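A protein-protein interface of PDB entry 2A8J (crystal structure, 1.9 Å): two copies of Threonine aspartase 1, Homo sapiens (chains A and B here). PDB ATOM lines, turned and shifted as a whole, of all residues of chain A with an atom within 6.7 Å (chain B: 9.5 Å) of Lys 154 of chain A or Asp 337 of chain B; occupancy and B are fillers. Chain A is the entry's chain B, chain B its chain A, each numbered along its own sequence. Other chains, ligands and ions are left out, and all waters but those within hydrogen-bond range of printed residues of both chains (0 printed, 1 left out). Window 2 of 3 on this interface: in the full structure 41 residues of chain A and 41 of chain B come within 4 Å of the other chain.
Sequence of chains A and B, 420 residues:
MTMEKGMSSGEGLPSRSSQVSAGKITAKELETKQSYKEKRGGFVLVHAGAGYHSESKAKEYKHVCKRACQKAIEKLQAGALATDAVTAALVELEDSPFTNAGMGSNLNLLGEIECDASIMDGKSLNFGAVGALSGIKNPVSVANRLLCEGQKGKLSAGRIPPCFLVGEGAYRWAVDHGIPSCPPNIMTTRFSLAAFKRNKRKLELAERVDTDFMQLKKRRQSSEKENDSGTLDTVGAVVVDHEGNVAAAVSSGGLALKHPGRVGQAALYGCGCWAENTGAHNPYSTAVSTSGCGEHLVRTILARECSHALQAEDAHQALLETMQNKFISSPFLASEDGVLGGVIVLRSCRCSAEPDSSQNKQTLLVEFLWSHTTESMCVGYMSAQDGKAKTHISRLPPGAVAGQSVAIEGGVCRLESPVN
The guanidinium group of Arg 262 of chain B lies within hydrogen-bond range of the backbone carbonyl oxygen of Pro 161 of chain A (3.4 Å).
O of Ile 160 of chain A is in hydrogen-bond range of NH2 of Arg 262 of chain B (3.0 Å).
The backbone carbonyl oxygen (O) of Pro 161 of chain A sits close to the side-chain carboxylate (OE1) of Glu 295 of chain B (3.2 Å).
The side-chain carboxylate (OE1) of Glu 295 of chain B is in salt-bridge range of the guanidinium group (NH2) of Arg 262 of chain B.
Among the printed residues, pairs that only touch across the chains: Ile 160 of chain A with Glu 295 of chain B, Lys 154 of chain A with Glu 336 of chain B and Lys 154 of chain A with Asp 337 of chain B.
Lys 154 of chain A touches two residues of chain B.
Asp 337 of chain B touches one residue of chain A.
No residue of chain B comes within 4 Å of Gly 153 of chain A.
Of the printed residues of chain A, Glu 295 of chain B touches Ile 160 and Pro 161.
Of the printed residues of chain A, Glu 336 of chain B touches Lys 154.
Printed residues of chain B within 4 Å of Pro 161 of chain A: Arg 262 (3.4 Å) and Glu 295 (3.2 Å).
Printed residues of chain B within 4 Å of Ile 160 of chain A: Arg 262 (3.0 Å) and Glu 295 (3.3 Å).
Of the printed residues of chain A, Arg 262 of chain B touches Ile 160 (3.0 Å) and Pro 161 (3.4 Å).
Glu 149 of chain A touches none of the printed residues of chain B.
The nearest printed residue of chain A that does not touch Glu 295 of chain B is Arg 159 of chain A (7.3 Å).
Hydrophobic or aromatic side chains of chain A within 4 Å of the printed part of chain B: Ile 160.
Of the 18 printed residues of chain B, 4 touch a printed residue of chain A.
Printed residues of chain B that touch a printed residue of chain A: Arg 262, Glu 295, Glu 336 and Asp 337.
No position is printed for both chains.
Of the 6 pairs that touch across the chains among the printed residues, none has its exchanged pair printed and touching as well.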
ATOM      1  N   GLU A 149      -7.659 -27.812 -26.344  1.00  0.00           N
ATOM      2  CA  GLU A 149      -8.965 -27.195 -26.179  1.00  0.00           C
ATOM      3  C   GLU A 149      -8.898 -25.947 -25.315  1.00  0.00           C
ATOM      4  O   GLU A 149      -9.557 -24.953 -25.605  1.00  0.00           O
ATOM      5  CB  GLU A 149      -9.949 -28.196 -25.578  1.00  0.00           C
ATOM      6  CG  GLU A 149     -10.402 -29.255 -26.563  1.00  0.00           C
ATOM      7  CD  GLU A 149     -11.191 -28.664 -27.722  1.00  0.00           C
ATOM      8  OE1 GLU A 149     -12.173 -27.936 -27.462  1.00  0.00           O
ATOM      9  OE2 GLU A 149     -10.831 -28.929 -28.887  1.00  0.00           O
ATOM     10  N   GLY A 150      -8.091 -25.999 -24.258  1.00  0.00           N
ATOM     11  CA  GLY A 150      -7.963 -24.854 -23.377  1.00  0.00           C
ATOM     12  C   GLY A 150      -7.381 -23.653 -24.098  1.00  0.00           C
ATOM     13  O   GLY A 150      -7.794 -22.517 -23.870  1.00  0.00           O
ATOM     14  N   LYS A 152      -7.835 -22.694 -27.018  1.00  0.00           N
ATOM     15  CA  LYS A 152      -8.824 -22.043 -27.873  1.00  0.00           C
ATOM     16  C   LYS A 152      -9.499 -20.874 -27.170  1.00  0.00           C
ATOM     17  O   LYS A 152      -9.828 -19.868 -27.803  1.00  0.00           O
ATOM     18  CB  LYS A 152      -9.894 -23.038 -28.318  1.00  0.00           C
ATOM     19  CG  LYS A 152      -9.368 -24.153 -29.184  1.00  0.00           C
ATOM     20  CD  LYS A 152     -10.482 -25.082 -29.596  1.00  0.00           C
ATOM     21  CE  LYS A 152      -9.951 -26.202 -30.467  1.00  0.00           C
ATOM     22  NZ  LYS A 152     -11.037 -27.141 -30.857  1.00  0.00           N
ATOM     23  N   GLY A 153      -9.716 -21.008 -25.865  1.00  0.00           N
ATOM     24  CA  GLY A 153     -10.352 -19.933 -25.127  1.00  0.00           C
ATOM     25  C   GLY A 153     -11.482 -20.378 -24.221  1.00  0.00           C
ATOM     26  O   GLY A 153     -11.847 -21.553 -24.185  1.00  0.00           O
ATOM     27  N   LYS A 154     -12.044 -19.421 -23.493  1.00  0.00           N
ATOM     28  CA  LYS A 154     -13.130 -19.687 -22.560  1.00  0.00           C
ATOM     29  C   LYS A 154     -14.353 -20.334 -23.203  1.00  0.00           C
ATOM     30  O   LYS A 154     -14.721 -20.015 -24.334  1.00  0.00           O
ATOM     31  CB  LYS A 154     -13.525 -18.387 -21.862  1.00  0.00           C
ATOM     32  CG  LYS A 154     -12.362 -17.746 -21.122  1.00  0.00           C
ATOM     33  CD  LYS A 154     -12.660 -16.321 -20.692  1.00  0.00           C
ATOM     34  CE  LYS A 154     -11.456 -15.724 -19.967  1.00  0.00           C
ATOM     35  NZ  LYS A 154     -11.657 -14.293 -19.598  1.00  0.00           N
ATOM     36  N   LEU A 155     -14.975 -21.247 -22.464  1.00  0.00           N
ATOM     37  CA  LEU A 155     -16.154 -21.957 -22.930  1.00  0.00           C
ATOM     38  C   LEU A 155     -17.416 -21.100 -22.866  1.00  0.00           C
ATOM     39  O   LEU A 155     -18.427 -21.429 -23.495  1.00  0.00           O
ATOM     40  CB  LEU A 155     -16.361 -23.225 -22.097  1.00  0.00           C
ATOM     41  CG  LEU A 155     -15.324 -24.341 -22.238  1.00  0.00           C
ATOM     42  CD1 LEU A 155     -15.635 -25.449 -21.241  1.00  0.00           C
ATOM     43  CD2 LEU A 155     -15.337 -24.881 -23.666  1.00  0.00           C
ATOM     44  N   SER A 156     -17.362 -20.010 -22.106  1.00  0.00           N
ATOM     45  CA  SER A 156     -18.521 -19.131 -21.968  1.00  0.00           C
ATOM     46  C   SER A 156     -18.131 -17.692 -21.648  1.00  0.00           C
ATOM     47  O   SER A 156     -18.843 -17.003 -20.914  1.00  0.00           O
ATOM     48  CB  SER A 156     -19.452 -19.651 -20.868  1.00  0.00           C
ATOM     49  OG  SER A 156     -20.004 -20.907 -21.218  1.00  0.00           O
ATOM     50  N   ARG A 159     -15.899 -18.753 -19.110  1.00  0.00           N
ATOM     51  CA  ARG A 159     -15.358 -19.763 -18.204  1.00  0.00           C
ATOM     52  C   ARG A 159     -14.174 -20.499 -18.808  1.00  0.00           C
ATOM     53  O   ARG A 159     -14.240 -20.970 -19.945  1.00  0.00           O
ATOM     54  CB  ARG A 159     -16.428 -20.788 -17.835  1.00  0.00           C
ATOM     55  CG  ARG A 159     -15.849 -22.025 -17.163  1.00  0.00           C
ATOM     56  CD  ARG A 159     -16.927 -23.029 -16.824  1.00  0.00           C
ATOM     57  NE  ARG A 159     -17.866 -22.492 -15.845  1.00  0.00           N
ATOM     58  CZ  ARG A 159     -18.926 -23.152 -15.391  1.00  0.00           C
ATOM     59  NH1 ARG A 159     -19.181 -24.378 -15.832  1.00  0.00           N
ATOM     60  NH2 ARG A 159     -19.731 -22.584 -14.500  1.00  0.00           N
ATOM     61  N   ILE A 160     -13.097 -20.613 -18.037  1.00  0.00           N
ATOM     62  CA  ILE A 160     -11.911 -21.305 -18.515  1.00  0.00           C
ATOM     63  C   ILE A 160     -12.219 -22.790 -18.655  1.00  0.00           C
ATOM     64  O   ILE A 160     -12.906 -23.378 -17.816  1.00  0.00           O
ATOM     65  CB  ILE A 160     -10.712 -21.107 -17.554  1.00  0.00           C
ATOM     66  CG1 ILE A 160      -9.516 -21.940 -18.030  1.00  0.00           C
ATOM     67  CG2 ILE A 160     -11.114 -21.477 -16.138  1.00  0.00           C
ATOM     68  CD1 ILE A 160      -8.248 -21.736 -17.220  1.00  0.00           C
ATOM     69  N   PRO A 161     -11.739 -23.409 -19.743  1.00  0.00           N
ATOM     70  CA  PRO A 161     -11.987 -24.833 -19.950  1.00  0.00           C
ATOM     71  C   PRO A 161     -11.277 -25.589 -18.837  1.00  0.00           C
ATOM     72  O   PRO A 161     -10.412 -25.039 -18.160  1.00  0.00           O
ATOM     73  CB  PRO A 161     -11.369 -25.101 -21.322  1.00  0.00           C
ATOM     74  CG  PRO A 161     -11.449 -23.762 -21.999  1.00  0.00           C
ATOM     75  CD  PRO A 161     -11.029 -22.831 -20.896  1.00  0.00           C
ATOM     76  N   TYR B  52     -18.269 -12.330  -5.883  1.00  0.00           N
ATOM     77  CA  TYR B  52     -19.058 -11.116  -5.974  1.00  0.00           C
ATOM     78  C   TYR B  52     -19.859 -10.844  -4.707  1.00  0.00           C
ATOM     79  O   TYR B  52     -20.416 -11.754  -4.090  1.00  0.00           O
ATOM     80  CB  TYR B  52     -19.933 -11.159  -7.227  1.00  0.00           C
ATOM     81  CG  TYR B  52     -19.233 -10.483  -8.393  1.00  0.00           C
ATOM     82  CD1 TYR B  52     -17.837 -10.523  -8.502  1.00  0.00           C
ATOM     83  CD2 TYR B  52     -19.946  -9.759  -9.349  1.00  0.00           C
ATOM     84  CE1 TYR B  52     -17.171  -9.851  -9.526  1.00  0.00           C
ATOM     85  CE2 TYR B  52     -19.287  -9.083 -10.383  1.00  0.00           C
ATOM     86  CZ  TYR B  52     -17.899  -9.132 -10.462  1.00  0.00           C
ATOM     87  OH  TYR B  52     -17.234  -8.445 -11.456  1.00  0.00           O
ATOM     88  N   ARG B 262     -14.098 -32.782 -13.229  1.00  0.00           N
ATOM     89  CA  ARG B 262     -13.250 -31.602 -13.180  1.00  0.00           C
ATOM     90  C   ARG B 262     -12.823 -31.315 -11.753  1.00  0.00           C
ATOM     91  O   ARG B 262     -13.667 -31.101 -10.878  1.00  0.00           O
ATOM     92  CB  ARG B 262     -13.980 -30.387 -13.737  1.00  0.00           C
ATOM     93  CG  ARG B 262     -13.131 -29.142 -13.692  1.00  0.00           C
ATOM     94  CD  ARG B 262     -13.808 -27.991 -14.380  1.00  0.00           C
ATOM     95  NE  ARG B 262     -12.946 -26.821 -14.432  1.00  0.00           N
ATOM     96  CZ  ARG B 262     -13.053 -25.863 -15.345  1.00  0.00           C
ATOM     97  NH1 ARG B 262     -13.979 -25.947 -16.287  1.00  0.00           N
ATOM     98  NH2 ARG B 262     -12.257 -24.808 -15.294  1.00  0.00           N
ATOM     99  N   CYS B 293     -11.268 -18.485  -8.528  1.00  0.00           N
ATOM    100  CA  CYS B 293     -11.210 -19.290  -9.741  1.00  0.00           C
ATOM    101  C   CYS B 293     -10.175 -20.405  -9.636  1.00  0.00           C
ATOM    102  O   CYS B 293      -8.975 -20.151  -9.664  1.00  0.00           O
ATOM    103  CB  CYS B 293     -10.879 -18.404 -10.944  1.00  0.00           C
ATOM    104  SG  CYS B 293     -10.636 -19.351 -12.458  1.00  0.00           S
ATOM    105  N   GLU B 295      -8.761 -22.697 -11.636  1.00  0.00           N
ATOM    106  CA  GLU B 295      -7.657 -22.732 -12.588  1.00  0.00           C
ATOM    107  C   GLU B 295      -6.589 -21.672 -12.326  1.00  0.00           C
ATOM    108  O   GLU B 295      -5.393 -21.941 -12.455  1.00  0.00           O
ATOM    109  CB  GLU B 295      -8.196 -22.582 -14.008  1.00  0.00           C
ATOM    110  CG  GLU B 295      -9.300 -23.581 -14.354  1.00  0.00           C
ATOM    111  CD  GLU B 295      -8.833 -25.026 -14.317  1.00  0.00           C
ATOM    112  OE1 GLU B 295      -8.937 -25.714 -15.359  1.00  0.00           O
ATOM    113  OE2 GLU B 295      -8.367 -25.481 -13.248  1.00  0.00           O
ATOM    114  N   HIS B 296      -7.023 -20.474 -11.947  1.00  0.00           N
ATOM    115  CA  HIS B 296      -6.096 -19.382 -11.684  1.00  0.00           C
ATOM    116  C   HIS B 296      -5.187 -19.669 -10.497  1.00  0.00           C
ATOM    117  O   HIS B 296      -4.000 -19.357 -10.535  1.00  0.00           O
ATOM    118  CB  HIS B 296      -6.866 -18.086 -11.426  1.00  0.00           C
ATOM    119  CG  HIS B 296      -7.596 -17.566 -12.624  1.00  0.00           C
ATOM    120  ND1 HIS B 296      -8.443 -16.480 -12.561  1.00  0.00           N
ATOM    121  CD2 HIS B 296      -7.622 -17.991 -13.910  1.00  0.00           C
ATOM    122  CE1 HIS B 296      -8.962 -16.260 -13.756  1.00  0.00           C
ATOM    123  NE2 HIS B 296      -8.480 -17.163 -14.594  1.00  0.00           N
ATOM    124  N   ILE B 328      -2.001 -11.576 -10.095  1.00  0.00           N
ATOM    125  CA  ILE B 328      -2.588 -10.704 -11.110  1.00  0.00           C
ATOM    126  C   ILE B 328      -1.712 -10.615 -12.354  1.00  0.00           C
ATOM    127  O   ILE B 328      -2.177 -10.885 -13.455  1.00  0.00           O
ATOM    128  CB  ILE B 328      -2.844  -9.275 -10.566  1.00  0.00           C
ATOM    129  CG1 ILE B 328      -4.013  -9.312  -9.576  1.00  0.00           C
ATOM    130  CG2 ILE B 328      -3.158  -8.309 -11.721  1.00  0.00           C
ATOM    131  CD1 ILE B 328      -4.308  -7.994  -8.910  1.00  0.00           C
ATOM    132  N   LEU B 333      -0.857 -16.502 -16.214  1.00  0.00           N
ATOM    133  CA  LEU B 333      -2.253 -16.104 -16.342  1.00  0.00           C
ATOM    134  C   LEU B 333      -2.407 -14.914 -17.287  1.00  0.00           C
ATOM    135  O   LEU B 333      -3.437 -14.235 -17.283  1.00  0.00           O
ATOM    136  CB  LEU B 333      -2.822 -15.744 -14.963  1.00  0.00           C
ATOM    137  CG  LEU B 333      -2.952 -16.876 -13.938  1.00  0.00           C
ATOM    138  CD1 LEU B 333      -3.546 -16.330 -12.647  1.00  0.00           C
ATOM    139  CD2 LEU B 333      -3.832 -17.975 -14.492  1.00  0.00           C
ATOM    140  N   ALA B 334      -1.382 -14.663 -18.094  1.00  0.00           N
ATOM    141  CA  ALA B 334      -1.399 -13.541 -19.027  1.00  0.00           C
ATOM    142  C   ALA B 334      -2.578 -13.551 -19.997  1.00  0.00           C
ATOM    143  O   ALA B 334      -3.131 -12.500 -20.319  1.00  0.00           O
ATOM    144  CB  ALA B 334      -0.085 -13.493 -19.804  1.00  0.00           C
ATOM    145  N   SER B 335      -2.963 -14.732 -20.463  1.00  0.00           N
ATOM    146  CA  SER B 335      -4.071 -14.841 -21.404  1.00  0.00           C
ATOM    147  C   SER B 335      -5.419 -14.585 -20.741  1.00  0.00           C
ATOM    148  O   SER B 335      -6.444 -14.490 -21.420  1.00  0.00           O
ATOM    149  CB  SER B 335      -4.081 -16.227 -22.055  1.00  0.00           C
ATOM    150  OG  SER B 335      -2.857 -16.485 -22.722  1.00  0.00           O
ATOM    151  N   GLU B 336      -5.423 -14.465 -19.417  1.00  0.00           N
ATOM    152  CA  GLU B 336      -6.670 -14.237 -18.712  1.00  0.00           C
ATOM    153  C   GLU B 336      -7.105 -12.793 -18.649  1.00  0.00           C
ATOM    154  O   GLU B 336      -6.305 -11.884 -18.425  1.00  0.00           O
ATOM    155  CB  GLU B 336      -6.610 -14.812 -17.293  1.00  0.00           C
ATOM    156  CG  GLU B 336      -6.601 -16.324 -17.275  1.00  0.00           C
ATOM    157  CD  GLU B 336      -7.530 -16.898 -18.326  1.00  0.00           C
ATOM    158  OE1 GLU B 336      -8.765 -16.712 -18.206  1.00  0.00           O
ATOM    159  OE2 GLU B 336      -7.018 -17.522 -19.282  1.00  0.00           O
ATOM    160  N   ASP B 337      -8.399 -12.598 -18.866  1.00  0.00           N
ATOM    161  CA  ASP B 337      -9.000 -11.280 -18.815  1.00  0.00           C
ATOM    162  C   ASP B 337      -9.587 -11.188 -17.413  1.00  0.00           C
ATOM    163  O   ASP B 337     -10.790 -11.371 -17.201  1.00  0.00           O
ATOM    164  CB  ASP B 337     -10.086 -11.166 -19.888  1.00  0.00           C
ATOM    165  CG  ASP B 337     -10.820  -9.849 -19.837  1.00  0.00           C
ATOM    166  OD1 ASP B 337     -10.183  -8.830 -19.492  1.00  0.00           O
ATOM    167  OD2 ASP B 337     -12.030  -9.831 -20.152  1.00  0.00           O
ATOM    168  N   GLY B 338      -8.711 -10.929 -16.452  1.00  0.00           N
ATOM    169  CA  GLY B 338      -9.128 -10.843 -15.068  1.00  0.00           C
ATOM    170  C   GLY B 338      -8.649 -12.075 -14.324  1.00  0.00           C
ATOM    171  O   GLY B 338      -8.781 -13.194 -14.818  1.00  0.00           O
ATOM    172  N   VAL B 339      -8.079 -11.859 -13.144  1.00  0.00           N
ATOM    173  CA  VAL B 339      -7.563 -12.934 -12.296  1.00  0.00           C
ATOM    174  C   VAL B 339      -8.334 -12.860 -10.979  1.00  0.00           C
ATOM    175  O   VAL B 339      -8.246 -11.866 -10.264  1.00  0.00           O
ATOM    176  CB  VAL B 339      -6.054 -12.734 -12.048  1.00  0.00           C
ATOM    177  CG1 VAL B 339      -5.499 -13.874 -11.225  1.00  0.00           C
ATOM    178  CG2 VAL B 339      -5.331 -12.643 -13.382  1.00  0.00           C
ATOM    179  N   LEU B 340      -9.081 -13.917 -10.665  1.00  0.00           N
ATOM    180  CA  LEU B 340      -9.925 -13.965  -9.469  1.00  0.00           C
ATOM    181  C   LEU B 340      -9.458 -14.935  -8.379  1.00  0.00           C
ATOM    182  O   LEU B 340      -9.407 -16.149  -8.578  1.00  0.00           O
ATOM    183  CB  LEU B 340     -11.360 -14.319  -9.892  1.00  0.00           C
ATOM    184  CG  LEU B 340     -11.974 -13.380 -10.947  1.00  0.00           C
ATOM    185  CD1 LEU B 340     -13.231 -14.011 -11.548  1.00  0.00           C
ATOM    186  CD2 LEU B 340     -12.296 -12.030 -10.310  1.00  0.00           C
ATOM    187  N   VAL B 401     -11.400  -2.429  -9.990  1.00  0.00           N
ATOM    188  CA  VAL B 401     -12.048  -3.423 -10.827  1.00  0.00           C
ATOM    189  C   VAL B 401     -11.704  -4.836 -10.363  1.00  0.00           C
ATOM    190  O   VAL B 401     -10.534  -5.177 -10.200  1.00  0.00           O
ATOM    191  CB  VAL B 401     -11.631  -3.266 -12.297  1.00  0.00           C
ATOM    192  CG1 VAL B 401     -12.382  -4.268 -13.158  1.00  0.00           C
ATOM    193  CG2 VAL B 401     -11.911  -1.845 -12.764  1.00  0.00           C
ATOM    194  N   ALA B 402     -12.732  -5.647 -10.152  1.00  0.00           N
ATOM    195  CA  ALA B 402     -12.535  -7.021  -9.717  1.00  0.00           C
ATOM    196  C   ALA B 402     -11.702  -7.764 -10.748  1.00  0.00           C
ATOM    197  O   ALA B 402     -11.907  -7.608 -11.950  1.00  0.00           O
ATOM    198  CB  ALA B 402     -13.882  -7.711  -9.536  1.00  0.00           C
ATOM    199  N   GLY B 403     -10.757  -8.565 -10.271  1.00  0.00           N
ATOM    200  CA  GLY B 403      -9.908  -9.331 -11.165  1.00  0.00           C
ATOM    201  C   GLY B 403      -8.762  -8.536 -11.760  1.00  0.00           C
ATOM    202  O   GLY B 403      -7.969  -9.078 -12.518  1.00  0.00           O
ATOM    203  N   GLN B 404      -8.674  -7.255 -11.416  1.00  0.00           N
ATOM    204  CA  GLN B 404      -7.620  -6.381 -11.934  1.00  0.00           C
ATOM    205  C   GLN B 404      -6.911  -5.636 -10.809  1.00  0.00           C
ATOM    206  O   GLN B 404      -5.861  -5.030 -11.022  1.00  0.00           O
ATOM    207  CB  GLN B 404      -8.207  -5.348 -12.904  1.00  0.00           C
ATOM    208  CG  GLN B 404      -8.792  -5.911 -14.190  1.00  0.00           C
ATOM    209  CD  GLN B 404      -7.742  -6.520 -15.102  1.00  0.00           C
ATOM    210  OE1 GLN B 404      -6.700  -5.911 -15.361  1.00  0.00           O
ATOM    211  NE2 GLN B 404      -8.014  -7.722 -15.605  1.00  0.00           N
